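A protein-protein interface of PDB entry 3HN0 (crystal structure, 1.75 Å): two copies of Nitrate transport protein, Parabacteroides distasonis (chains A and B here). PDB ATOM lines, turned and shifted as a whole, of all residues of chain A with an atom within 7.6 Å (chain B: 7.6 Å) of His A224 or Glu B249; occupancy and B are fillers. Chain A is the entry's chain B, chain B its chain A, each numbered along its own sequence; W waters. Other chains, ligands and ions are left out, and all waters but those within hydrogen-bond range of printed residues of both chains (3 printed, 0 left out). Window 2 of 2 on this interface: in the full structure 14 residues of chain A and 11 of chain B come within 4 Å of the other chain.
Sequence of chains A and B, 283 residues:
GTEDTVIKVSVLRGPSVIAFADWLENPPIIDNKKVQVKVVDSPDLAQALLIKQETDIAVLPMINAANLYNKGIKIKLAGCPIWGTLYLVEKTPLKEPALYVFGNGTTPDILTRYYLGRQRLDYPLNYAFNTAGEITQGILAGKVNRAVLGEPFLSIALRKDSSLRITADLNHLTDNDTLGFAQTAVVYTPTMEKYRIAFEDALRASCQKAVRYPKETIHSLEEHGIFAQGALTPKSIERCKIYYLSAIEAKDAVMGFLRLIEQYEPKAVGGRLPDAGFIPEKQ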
ATOM      1  N   ALA A  21       2.959  -0.032 -20.290  1.00  0.00           N
ATOM      2  CA  ALA A  21       4.196  -0.684 -19.929  1.00  0.00           C
ATOM      3  C   ALA A  21       4.689  -0.388 -18.510  1.00  0.00           C
ATOM      4  O   ALA A  21       5.183  -1.289 -17.818  1.00  0.00           O
ATOM      5  CB  ALA A  21       5.308  -0.349 -20.931  1.00  0.00           C
ATOM      6  N   TRP A  23       3.176  -0.031 -15.850  1.00  0.00           N
ATOM      7  CA  TRP A  23       2.423  -0.804 -14.861  1.00  0.00           C
ATOM      8  C   TRP A  23       2.848  -2.249 -14.735  1.00  0.00           C
ATOM      9  O   TRP A  23       2.443  -2.928 -13.769  1.00  0.00           O
ATOM     10  CB  TRP A  23       0.918  -0.709 -15.155  1.00  0.00           C
ATOM     11  CG  TRP A  23       0.388   0.670 -15.082  1.00  0.00           C
ATOM     12  CD1 TRP A  23       1.066   1.798 -14.727  1.00  0.00           C
ATOM     13  CD2 TRP A  23      -0.956   1.069 -15.290  1.00  0.00           C
ATOM     14  NE1 TRP A  23       0.230   2.874 -14.756  1.00  0.00           N
ATOM     15  CE2 TRP A  23      -1.016   2.461 -15.109  1.00  0.00           C
ATOM     16  CE3 TRP A  23      -2.127   0.381 -15.642  1.00  0.00           C
ATOM     17  CZ2 TRP A  23      -2.189   3.176 -15.245  1.00  0.00           C
ATOM     18  CZ3 TRP A  23      -3.292   1.072 -15.766  1.00  0.00           C
ATOM     19  CH2 TRP A  23      -3.330   2.476 -15.580  1.00  0.00           C
ATOM     20  N   LEU A  24       3.691  -2.719 -15.652  1.00  0.00           N
ATOM     21  CA  LEU A  24       4.318  -4.021 -15.505  1.00  0.00           C
ATOM     22  C   LEU A  24       5.196  -4.065 -14.281  1.00  0.00           C
ATOM     23  O   LEU A  24       5.204  -5.087 -13.594  1.00  0.00           O
ATOM     24  CB  LEU A  24       5.192  -4.395 -16.724  1.00  0.00           C
ATOM     25  CG  LEU A  24       4.368  -4.533 -18.005  1.00  0.00           C
ATOM     26  CD1 LEU A  24       5.264  -4.902 -19.209  1.00  0.00           C
ATOM     27  CD2 LEU A  24       3.203  -5.529 -17.855  1.00  0.00           C
ATOM     28  N   GLU A  25       6.026  -3.034 -14.083  1.00  0.00           N
ATOM     29  CA  GLU A  25       6.908  -2.977 -12.895  1.00  0.00           C
ATOM     30  C   GLU A  25       6.305  -2.110 -11.815  1.00  0.00           C
ATOM     31  O   GLU A  25       6.522  -2.346 -10.623  1.00  0.00           O
ATOM     32  CB  GLU A  25       8.297  -2.449 -13.267  1.00  0.00           C
ATOM     33  CG  GLU A  25       9.055  -3.418 -14.196  1.00  0.00           C
ATOM     34  CD  GLU A  25      10.398  -2.907 -14.708  1.00  0.00           C
ATOM     35  OE1 GLU A  25      10.776  -1.758 -14.425  1.00  0.00           O
ATOM     36  OE2 GLU A  25      11.087  -3.678 -15.414  1.00  0.00           O
ATOM     37  N   ASN A  26       5.548  -1.097 -12.216  1.00  0.00           N
ATOM     38  CA  ASN A  26       5.072  -0.112 -11.236  1.00  0.00           C
ATOM     39  C   ASN A  26       3.555   0.021 -11.264  1.00  0.00           C
ATOM     40  O   ASN A  26       3.036   1.063 -11.578  1.00  0.00           O
ATOM     41  CB  ASN A  26       5.773   1.205 -11.482  1.00  0.00           C
ATOM     42  CG  ASN A  26       7.273   1.041 -11.555  1.00  0.00           C
ATOM     43  OD1 ASN A  26       7.898   0.581 -10.602  1.00  0.00           O
ATOM     44  ND2 ASN A  26       7.856   1.413 -12.683  1.00  0.00           N
ATOM     45  N   VAL A  39      -2.174  -9.268 -19.774  1.00  0.00           N
ATOM     46  CA  VAL A  39      -2.128  -9.137 -21.191  1.00  0.00           C
ATOM     47  C   VAL A  39      -2.867 -10.347 -21.770  1.00  0.00           C
ATOM     48  O   VAL A  39      -2.603 -11.492 -21.378  1.00  0.00           O
ATOM     49  CB  VAL A  39      -0.628  -9.106 -21.658  1.00  0.00           C
ATOM     50  CG1 VAL A  39      -0.529  -9.199 -23.172  1.00  0.00           C
ATOM     51  CG2 VAL A  39       0.054  -7.884 -21.137  1.00  0.00           C
ATOM     52  N   THR A 217      11.325   1.825 -21.423  1.00  0.00           N
ATOM     53  CA  THR A 217      10.017   1.217 -21.720  1.00  0.00           C
ATOM     54  C   THR A 217      10.156  -0.059 -22.546  1.00  0.00           C
ATOM     55  O   THR A 217       9.603  -1.106 -22.181  1.00  0.00           O
ATOM     56  CB  THR A 217       9.120   2.239 -22.418  1.00  0.00           C
ATOM     57  OG1 THR A 217       8.901   3.350 -21.526  1.00  0.00           O
ATOM     58  CG2 THR A 217       7.773   1.608 -22.832  1.00  0.00           C
ATOM     59  N   ILE A 218      10.892   0.030 -23.646  1.00  0.00           N
ATOM     60  CA  ILE A 218      11.176  -1.111 -24.498  1.00  0.00           C
ATOM     61  C   ILE A 218      11.882  -2.215 -23.705  1.00  0.00           C
ATOM     62  O   ILE A 218      11.517  -3.377 -23.814  1.00  0.00           O
ATOM     63  CB  ILE A 218      11.992  -0.698 -25.701  1.00  0.00           C
ATOM     64  CG1 ILE A 218      11.113   0.196 -26.599  1.00  0.00           C
ATOM     65  CG2 ILE A 218      12.530  -1.937 -26.434  1.00  0.00           C
ATOM     66  CD1 ILE A 218      11.840   1.000 -27.593  1.00  0.00           C
ATOM     67  N   HIS A 219      12.880  -1.856 -22.912  1.00  0.00           N
ATOM     68  CA  HIS A 219      13.593  -2.848 -22.104  1.00  0.00           C
ATOM     69  C   HIS A 219      12.644  -3.577 -21.151  1.00  0.00           C
ATOM     70  O   HIS A 219      12.702  -4.799 -21.055  1.00  0.00           O
ATOM     71  CB  HIS A 219      14.730  -2.217 -21.337  1.00  0.00           C
ATOM     72  CG  HIS A 219      15.985  -2.066 -22.141  1.00  0.00           C
ATOM     73  ND1 HIS A 219      16.144  -2.625 -23.399  1.00  0.00           N
ATOM     74  CD2 HIS A 219      17.161  -1.459 -21.849  1.00  0.00           C
ATOM     75  CE1 HIS A 219      17.355  -2.349 -23.852  1.00  0.00           C
ATOM     76  NE2 HIS A 219      17.994  -1.644 -22.932  1.00  0.00           N
ATOM     77  N   SER A 220      11.745  -2.851 -20.503  1.00  0.00           N
ATOM     78  CA  SER A 220      10.772  -3.496 -19.603  1.00  0.00           C
ATOM     79  C   SER A 220       9.866  -4.446 -20.386  1.00  0.00           C
ATOM     80  O   SER A 220       9.642  -5.590 -19.957  1.00  0.00           O
ATOM     81  CB  SER A 220       9.909  -2.483 -18.878  1.00  0.00           C
ATOM     82  OG  SER A 220       8.974  -3.173 -18.062  1.00  0.00           O
ATOM     83  N   LEU A 221       9.362  -3.979 -21.522  1.00  0.00           N
ATOM     84  CA  LEU A 221       8.510  -4.820 -22.393  1.00  0.00           C
ATOM     85  C   LEU A 221       9.220  -6.105 -22.843  1.00  0.00           C
ATOM     86  O   LEU A 221       8.610  -7.183 -22.887  1.00  0.00           O
ATOM     87  CB  LEU A 221       8.045  -4.045 -23.607  1.00  0.00           C
ATOM     88  CG  LEU A 221       6.972  -2.978 -23.314  1.00  0.00           C
ATOM     89  CD1 LEU A 221       6.863  -2.000 -24.493  1.00  0.00           C
ATOM     90  CD2 LEU A 221       5.600  -3.590 -22.958  1.00  0.00           C
ATOM     91  N   GLU A 222      10.505  -6.002 -23.172  1.00  0.00           N
ATOM     92  CA  GLU A 222      11.297  -7.160 -23.559  1.00  0.00           C
ATOM     93  C   GLU A 222      11.506  -8.103 -22.398  1.00  0.00           C
ATOM     94  O   GLU A 222      11.348  -9.317 -22.561  1.00  0.00           O
ATOM     95  CB  GLU A 222      12.639  -6.733 -24.201  1.00  0.00           C
ATOM     96  CG  GLU A 222      12.401  -6.019 -25.546  1.00  0.00           C
ATOM     97  CD  GLU A 222      13.654  -5.360 -26.144  1.00  0.00           C
ATOM     98  OE1 GLU A 222      14.645  -5.231 -25.433  1.00  0.00           O
ATOM     99  OE2 GLU A 222      13.604  -4.961 -27.328  1.00  0.00           O
ATOM    100  N   GLU A 223      11.875  -7.551 -21.249  1.00  0.00           N
ATOM    101  CA  GLU A 223      12.173  -8.362 -20.049  1.00  0.00           C
ATOM    102  C   GLU A 223      10.950  -9.073 -19.510  1.00  0.00           C
ATOM    103  O   GLU A 223      11.110 -10.110 -18.837  1.00  0.00           O
ATOM    104  CB  GLU A 223      12.804  -7.522 -18.946  1.00  0.00           C
ATOM    105  CG  GLU A 223      14.190  -6.996 -19.264  1.00  0.00           C
ATOM    106  CD  GLU A 223      14.545  -5.733 -18.438  1.00  0.00           C
ATOM    107  OE1 GLU A 223      13.836  -5.462 -17.454  1.00  0.00           O
ATOM    108  OE2 GLU A 223      15.537  -5.034 -18.769  1.00  0.00           O
ATOM    109  N   HIS A 224       9.757  -8.565 -19.817  1.00  0.00           N
ATOM    110  CA  HIS A 224       8.478  -9.256 -19.466  1.00  0.00           C
ATOM    111  C   HIS A 224       7.891 -10.093 -20.569  1.00  0.00           C
ATOM    112  O   HIS A 224       6.750 -10.535 -20.484  1.00  0.00           O
ATOM    113  CB  HIS A 224       7.457  -8.210 -18.981  1.00  0.00           C
ATOM    114  CG  HIS A 224       7.853  -7.578 -17.699  1.00  0.00           C
ATOM    115  ND1 HIS A 224       8.670  -6.470 -17.639  1.00  0.00           N
ATOM    116  CD2 HIS A 224       7.597  -7.928 -16.417  1.00  0.00           C
ATOM    117  CE1 HIS A 224       8.910  -6.173 -16.374  1.00  0.00           C
ATOM    118  NE2 HIS A 224       8.255  -7.031 -15.613  1.00  0.00           N
ATOM    119  N   GLY A 225       8.649 -10.304 -21.632  1.00  0.00           N
ATOM    120  CA  GLY A 225       8.174 -11.116 -22.731  1.00  0.00           C
ATOM    121  C   GLY A 225       6.948 -10.588 -23.466  1.00  0.00           C
ATOM    122  O   GLY A 225       6.188 -11.361 -24.029  1.00  0.00           O
ATOM    123  N   ILE A 226       6.747  -9.273 -23.526  1.00  0.00           N
ATOM    124  CA  ILE A 226       5.581  -8.756 -24.291  1.00  0.00           C
ATOM    125  C   ILE A 226       5.904  -8.613 -25.768  1.00  0.00           C
ATOM    126  O   ILE A 226       5.097  -8.931 -26.678  1.00  0.00           O
ATOM    127  CB  ILE A 226       5.086  -7.402 -23.696  1.00  0.00           C
ATOM    128  CG1 ILE A 226       4.832  -7.483 -22.182  1.00  0.00           C
ATOM    129  CG2 ILE A 226       3.844  -6.912 -24.465  1.00  0.00           C
ATOM    130  CD1 ILE A 226       3.962  -8.678 -21.719  1.00  0.00           C
ATOM    131  N   PHE A 227       7.125  -8.138 -26.046  1.00  0.00           N
ATOM    132  CA  PHE A 227       7.616  -8.062 -27.375  1.00  0.00           C
ATOM    133  C   PHE A 227       8.930  -8.768 -27.439  1.00  0.00           C
ATOM    134  O   PHE A 227       9.671  -8.729 -26.438  1.00  0.00           O
ATOM    135  CB  PHE A 227       7.793  -6.615 -27.793  1.00  0.00           C
ATOM    136  CG  PHE A 227       6.486  -5.878 -27.973  1.00  0.00           C
ATOM    137  CD1 PHE A 227       5.787  -5.977 -29.172  1.00  0.00           C
ATOM    138  CD2 PHE A 227       5.965  -5.103 -26.964  1.00  0.00           C
ATOM    139  CE1 PHE A 227       4.575  -5.294 -29.336  1.00  0.00           C
ATOM    140  CE2 PHE A 227       4.731  -4.424 -27.148  1.00  0.00           C
ATOM    141  CZ  PHE A 227       4.074  -4.539 -28.329  1.00  0.00           C
ATOM    142  N   ALA B  78      14.589 -22.663 -14.987  1.00  0.00           N
ATOM    143  CA  ALA B  78      15.090 -21.296 -14.883  1.00  0.00           C
ATOM    144  C   ALA B  78      14.423 -20.377 -15.898  1.00  0.00           C
ATOM    145  O   ALA B  78      13.948 -19.299 -15.541  1.00  0.00           O
ATOM    146  CB  ALA B  78      16.658 -21.229 -15.011  1.00  0.00           C
ATOM    147  N   TRP B  83      14.378 -18.618 -29.063  1.00  0.00           N
ATOM    148  CA  TRP B  83      12.972 -18.452 -29.409  1.00  0.00           C
ATOM    149  C   TRP B  83      12.668 -18.757 -30.898  1.00  0.00           C
ATOM    150  O   TRP B  83      11.526 -18.735 -31.327  1.00  0.00           O
ATOM    151  CB  TRP B  83      12.515 -17.021 -29.024  1.00  0.00           C
ATOM    152  CG  TRP B  83      12.694 -16.815 -27.534  1.00  0.00           C
ATOM    153  CD1 TRP B  83      13.830 -16.425 -26.904  1.00  0.00           C
ATOM    154  CD2 TRP B  83      11.746 -17.148 -26.501  1.00  0.00           C
ATOM    155  NE1 TRP B  83      13.665 -16.454 -25.545  1.00  0.00           N
ATOM    156  CE2 TRP B  83      12.375 -16.856 -25.259  1.00  0.00           C
ATOM    157  CE3 TRP B  83      10.416 -17.601 -26.502  1.00  0.00           C
ATOM    158  CZ2 TRP B  83      11.758 -17.050 -24.054  1.00  0.00           C
ATOM    159  CZ3 TRP B  83       9.776 -17.768 -25.280  1.00  0.00           C
ATOM    160  CH2 TRP B  83      10.465 -17.511 -24.055  1.00  0.00           C
ATOM    161  N   LEU B 179       6.811 -12.867 -29.463  1.00  0.00           N
ATOM    162  CA  LEU B 179       7.748 -13.630 -28.617  1.00  0.00           C
ATOM    163  C   LEU B 179       7.860 -15.069 -29.111  1.00  0.00           C
ATOM    164  O   LEU B 179       8.961 -15.594 -29.258  1.00  0.00           O
ATOM    165  CB  LEU B 179       7.339 -13.631 -27.133  1.00  0.00           C
ATOM    166  CG  LEU B 179       8.214 -14.458 -26.177  1.00  0.00           C
ATOM    167  CD1 LEU B 179       9.610 -13.917 -26.155  1.00  0.00           C
ATOM    168  CD2 LEU B 179       7.676 -14.553 -24.716  1.00  0.00           C
ATOM    169  N   ARG B 204      22.366 -13.931 -19.636  1.00  0.00           N
ATOM    170  CA  ARG B 204      21.942 -12.718 -20.341  1.00  0.00           C
ATOM    171  C   ARG B 204      23.103 -12.086 -21.090  1.00  0.00           C
ATOM    172  O   ARG B 204      22.951 -11.679 -22.220  1.00  0.00           O
ATOM    173  CB  ARG B 204      21.337 -11.707 -19.394  1.00  0.00           C
ATOM    174  CG  ARG B 204      19.988 -12.068 -18.907  1.00  0.00           C
ATOM    175  CD  ARG B 204      19.341 -10.930 -17.999  1.00  0.00           C
ATOM    176  NE  ARG B 204      18.170 -11.516 -17.360  1.00  0.00           N
ATOM    177  CZ  ARG B 204      18.116 -12.013 -16.142  1.00  0.00           C
ATOM    178  NH1 ARG B 204      19.081 -11.813 -15.251  1.00  0.00           N
ATOM    179  NH2 ARG B 204      17.022 -12.629 -15.755  1.00  0.00           N
ATOM    180  N   TYR B 243      17.722 -14.775 -26.726  1.00  0.00           N
ATOM    181  CA  TYR B 243      17.408 -13.846 -25.646  1.00  0.00           C
ATOM    182  C   TYR B 243      16.946 -14.638 -24.443  1.00  0.00           C
ATOM    183  O   TYR B 243      16.086 -15.516 -24.577  1.00  0.00           O
ATOM    184  CB  TYR B 243      16.285 -12.917 -26.061  1.00  0.00           C
ATOM    185  CG  TYR B 243      15.966 -11.817 -25.071  1.00  0.00           C
ATOM    186  CD1 TYR B 243      16.756 -10.680 -24.997  1.00  0.00           C
ATOM    187  CD2 TYR B 243      14.852 -11.882 -24.222  1.00  0.00           C
ATOM    188  CE1 TYR B 243      16.455  -9.638 -24.122  1.00  0.00           C
ATOM    189  CE2 TYR B 243      14.548 -10.831 -23.349  1.00  0.00           C
ATOM    190  CZ  TYR B 243      15.353  -9.712 -23.307  1.00  0.00           C
ATOM    191  OH  TYR B 243      15.072  -8.671 -22.423  1.00  0.00           O
ATOM    192  N   TYR B 244      17.474 -14.327 -23.273  1.00  0.00           N
ATOM    193  CA  TYR B 244      17.087 -15.084 -22.098  1.00  0.00           C
ATOM    194  C   TYR B 244      15.916 -14.407 -21.370  1.00  0.00           C
ATOM    195  O   TYR B 244      15.999 -13.234 -20.977  1.00  0.00           O
ATOM    196  CB  TYR B 244      18.281 -15.306 -21.150  1.00  0.00           C
ATOM    197  CG  TYR B 244      17.853 -16.107 -19.963  1.00  0.00           C
ATOM    198  CD1 TYR B 244      17.677 -17.457 -20.065  1.00  0.00           C
ATOM    199  CD2 TYR B 244      17.552 -15.489 -18.763  1.00  0.00           C
ATOM    200  CE1 TYR B 244      17.239 -18.194 -18.989  1.00  0.00           C
ATOM    201  CE2 TYR B 244      17.177 -16.229 -17.667  1.00  0.00           C
ATOM    202  CZ  TYR B 244      16.981 -17.558 -17.791  1.00  0.00           C
ATOM    203  OH  TYR B 244      16.585 -18.338 -16.725  1.00  0.00           O
ATOM    204  N   LEU B 245      14.835 -15.158 -21.182  1.00  0.00           N
ATOM    205  CA  LEU B 245      13.776 -14.795 -20.264  1.00  0.00           C
ATOM    206  C   LEU B 245      13.648 -15.828 -19.172  1.00  0.00           C
ATOM    207  O   LEU B 245      13.596 -17.067 -19.440  1.00  0.00           O
ATOM    208  CB  LEU B 245      12.415 -14.704 -20.979  1.00  0.00           C
ATOM    209  CG  LEU B 245      12.175 -13.512 -21.861  1.00  0.00           C
ATOM    210  CD1 LEU B 245      10.788 -13.734 -22.511  1.00  0.00           C
ATOM    211  CD2 LEU B 245      12.184 -12.206 -21.063  1.00  0.00           C
ATOM    212  N   SER B 246      13.571 -15.328 -17.938  1.00  0.00           N
ATOM    213  CA  SER B 246      13.272 -16.135 -16.768  1.00  0.00           C
ATOM    214  C   SER B 246      11.890 -16.755 -16.902  1.00  0.00           C
ATOM    215  O   SER B 246      10.994 -16.121 -17.447  1.00  0.00           O
ATOM    216  CB  SER B 246      13.271 -15.249 -15.519  1.00  0.00           C
ATOM    217  OG  SER B 246      12.764 -15.957 -14.405  1.00  0.00           O
ATOM    218  N   ALA B 247      11.699 -17.938 -16.340  1.00  0.00           N
ATOM    219  CA  ALA B 247      10.427 -18.622 -16.355  1.00  0.00           C
ATOM    220  C   ALA B 247       9.340 -17.797 -15.680  1.00  0.00           C
ATOM    221  O   ALA B 247       8.202 -17.890 -16.026  1.00  0.00           O
ATOM    222  CB  ALA B 247      10.576 -19.932 -15.600  1.00  0.00           C
ATOM    223  N   ILE B 248       9.697 -17.040 -14.660  1.00  0.00           N
ATOM    224  CA  ILE B 248       8.708 -16.191 -13.977  1.00  0.00           C
ATOM    225  C   ILE B 248       8.151 -15.197 -15.001  1.00  0.00           C
ATOM    226  O   ILE B 248       6.918 -15.064 -15.180  1.00  0.00           O
ATOM    227  CB  ILE B 248       9.302 -15.425 -12.775  1.00  0.00           C
ATOM    228  CG1 ILE B 248       9.667 -16.390 -11.631  1.00  0.00           C
ATOM    229  CG2 ILE B 248       8.303 -14.391 -12.296  1.00  0.00           C
ATOM    230  CD1 ILE B 248      11.051 -16.085 -10.889  1.00  0.00           C
ATOM    231  N   GLU B 249       9.037 -14.541 -15.735  1.00  0.00           N
ATOM    232  CA  GLU B 249       8.640 -13.538 -16.751  1.00  0.00           C
ATOM    233  C   GLU B 249       7.969 -14.161 -17.956  1.00  0.00           C
ATOM    234  O   GLU B 249       7.189 -13.508 -18.653  1.00  0.00           O
ATOM    235  CB  GLU B 249       9.867 -12.756 -17.216  1.00  0.00           C
ATOM    236  CG  GLU B 249      10.716 -12.134 -16.077  1.00  0.00           C
ATOM    237  CD  GLU B 249       9.880 -11.343 -15.104  1.00  0.00           C
ATOM    238  OE1 GLU B 249       8.824 -10.823 -15.530  1.00  0.00           O
ATOM    239  OE2 GLU B 249      10.275 -11.235 -13.919  1.00  0.00           O
ATOM    240  N   ALA B 250       8.292 -15.406 -18.248  1.00  0.00           N
ATOM    241  CA  ALA B 250       7.779 -16.058 -19.442  1.00  0.00           C
ATOM    242  C   ALA B 250       6.737 -17.139 -19.117  1.00  0.00           C
ATOM    243  O   ALA B 250       6.485 -18.033 -19.956  1.00  0.00           O
ATOM    244  CB  ALA B 250       8.967 -16.688 -20.228  1.00  0.00           C
ATOM    245  N   LYS B 251       6.113 -17.042 -17.938  1.00  0.00           N
ATOM    246  CA  LYS B 251       5.264 -18.121 -17.433  1.00  0.00           C
ATOM    247  C   LYS B 251       4.157 -18.395 -18.441  1.00  0.00           C
ATOM    248  O   LYS B 251       3.820 -19.553 -18.737  1.00  0.00           O
ATOM    249  CB  LYS B 251       4.684 -17.774 -16.047  1.00  0.00           C
ATOM    250  CG  LYS B 251       3.737 -18.873 -15.449  1.00  0.00           C
ATOM    251  CD  LYS B 251       3.175 -18.493 -14.082  1.00  0.00           C
ATOM    252  N   ASP B 252       3.608 -17.329 -19.033  1.00  0.00           N
ATOM    253  CA  ASP B 252       2.523 -17.515 -19.997  1.00  0.00           C
ATOM    254  C   ASP B 252       2.934 -18.188 -21.277  1.00  0.00           C
ATOM    255  O   ASP B 252       2.183 -19.025 -21.779  1.00  0.00           O
ATOM    256  CB  ASP B 252       1.764 -16.184 -20.250  1.00  0.00           C
ATOM    257  CG  ASP B 252       0.932 -15.731 -19.027  1.00  0.00           C
ATOM    258  OD1 ASP B 252       0.683 -16.523 -18.076  1.00  0.00           O
ATOM    259  OD2 ASP B 252       0.507 -14.543 -19.009  1.00  0.00           O
ATOM    260  N   ALA B 253       4.114 -17.858 -21.817  1.00  0.00           N
ATOM    261  CA  ALA B 253       4.684 -18.554 -22.965  1.00  0.00           C
ATOM    262  C   ALA B 253       5.092 -20.002 -22.647  1.00  0.00           C
ATOM    263  O   ALA B 253       5.229 -20.826 -23.568  1.00  0.00           O
ATOM    264  CB  ALA B 253       5.904 -17.806 -23.524  1.00  0.00           C
ATOM    265  N   VAL B 254       5.392 -20.272 -21.379  1.00  0.00           N
ATOM    266  CA  VAL B 254       5.764 -21.641 -20.982  1.00  0.00           C
ATOM    267  C   VAL B 254       4.512 -22.473 -20.903  1.00  0.00           C
ATOM    268  O   VAL B 254       4.378 -23.456 -21.601  1.00  0.00           O
ATOM    269  CB  VAL B 254       6.534 -21.689 -19.655  1.00  0.00           C
ATOM    270  CG1 VAL B 254       6.642 -23.165 -19.131  1.00  0.00           C
ATOM    271  CG2 VAL B 254       7.926 -21.050 -19.848  1.00  0.00           C
ATOM    272  N   ILE B 279       8.423 -23.727 -11.533  1.00  0.00           N
ATOM    273  CA  ILE B 279       9.052 -22.396 -11.679  1.00  0.00           C
ATOM    274  C   ILE B 279       9.418 -21.830 -10.287  1.00  0.00           C
ATOM    275  O   ILE B 279       8.603 -21.868  -9.401  1.00  0.00           O
ATOM    276  CB  ILE B 279       8.109 -21.513 -12.467  1.00  0.00           C
ATOM    277  CG1 ILE B 279       8.018 -22.073 -13.906  1.00  0.00           C
ATOM    278  CG2 ILE B 279       8.562 -20.019 -12.483  1.00  0.00           C
ATOM    279  CD1 ILE B 279       6.935 -21.519 -14.721  1.00  0.00           C
ATOM    280  N   LYS B 282       8.989 -15.869  -6.758  1.00  0.00           N
ATOM    281  CA  LYS B 282       9.594 -14.543  -7.007  1.00  0.00           C
ATOM    282  C   LYS B 282      10.505 -14.076  -5.850  1.00  0.00           C
ATOM    283  O   LYS B 282      11.529 -13.417  -6.102  1.00  0.00           O
ATOM    284  CB  LYS B 282       8.496 -13.500  -7.287  1.00  0.00           C
HETATM  285  O   HOH W   1       5.144 -12.695 -20.533  1.00  0.00           O
HETATM  286  O   HOH W   2      16.031  -6.304 -23.354  1.00  0.00           O
HETATM  287  O   HOH W   3       5.950 -10.963 -17.277  1.00  0.00           O
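The backbone carbonyl oxygen (O) of Tyr B243 sits at hydrogen-bond distance from the indole nitrogen (NE1) of Trp B83 (2.8 Å).
ND1 of His A224 sits at hydrogen-bond distance from O of Ser A220, 2.7 Å away.
Among the printed residues, merely in contact across the chains: Glu A222 with Tyr B243, Glu A222 with Leu B245, Glu A223 with Tyr B243, Glu A223 with Leu B245, Glu A223 with Glu B249, His A224 with Glu B249, Gly A225 with Leu B179 and Gly A225 with Leu B245.
Printed residues of chain B within 4 Å of Glu A222: Tyr B243 and Leu B245.
Of chain B, only Glu B249 (3.3 Å) comes within 4 Å of His A224.
Ile A226 touches none of the printed residues of chain B.
Printed residues of chain A within 4 Å of Leu B179: Gly A225 (3.6 Å).
The nearest residue of chain B that does not touch His A224 is Leu B245 (4.5 Å).
The nearest printed residue of chain B that does not touch Glu A223 is Ser B246 (5.8 Å).
Of the 18 printed residues of chain B, 4 touch a printed residue of chain A.
Hydrophobic or aromatic side chains of chain B that line the printed part of chain A: Leu B179, Tyr B243 and Leu B245.
Among the printed residues, 8 pairs touch across the chains.
Among the printed residues, no Asp or Glu carboxylate lies within 4 Å of a Lys or Arg side-chain nitrogen of the other chain.
No position is printed for both chains.
Water W1 lies within hydrogen-bond range of the backbone carbonyl oxygen (O) of His A224 (2.7 Å) and the backbone carbonyl oxygen (O) of Glu B249 (2.9 Å).
Water W2 bridges the side-chain hydroxyl (OH) of Tyr B243 and the side-chain carboxylate (OE1) of Glu A222.
Water W3 bridges O of Glu B249 (3.1 Å) and O of His A224 (3.3 Å).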
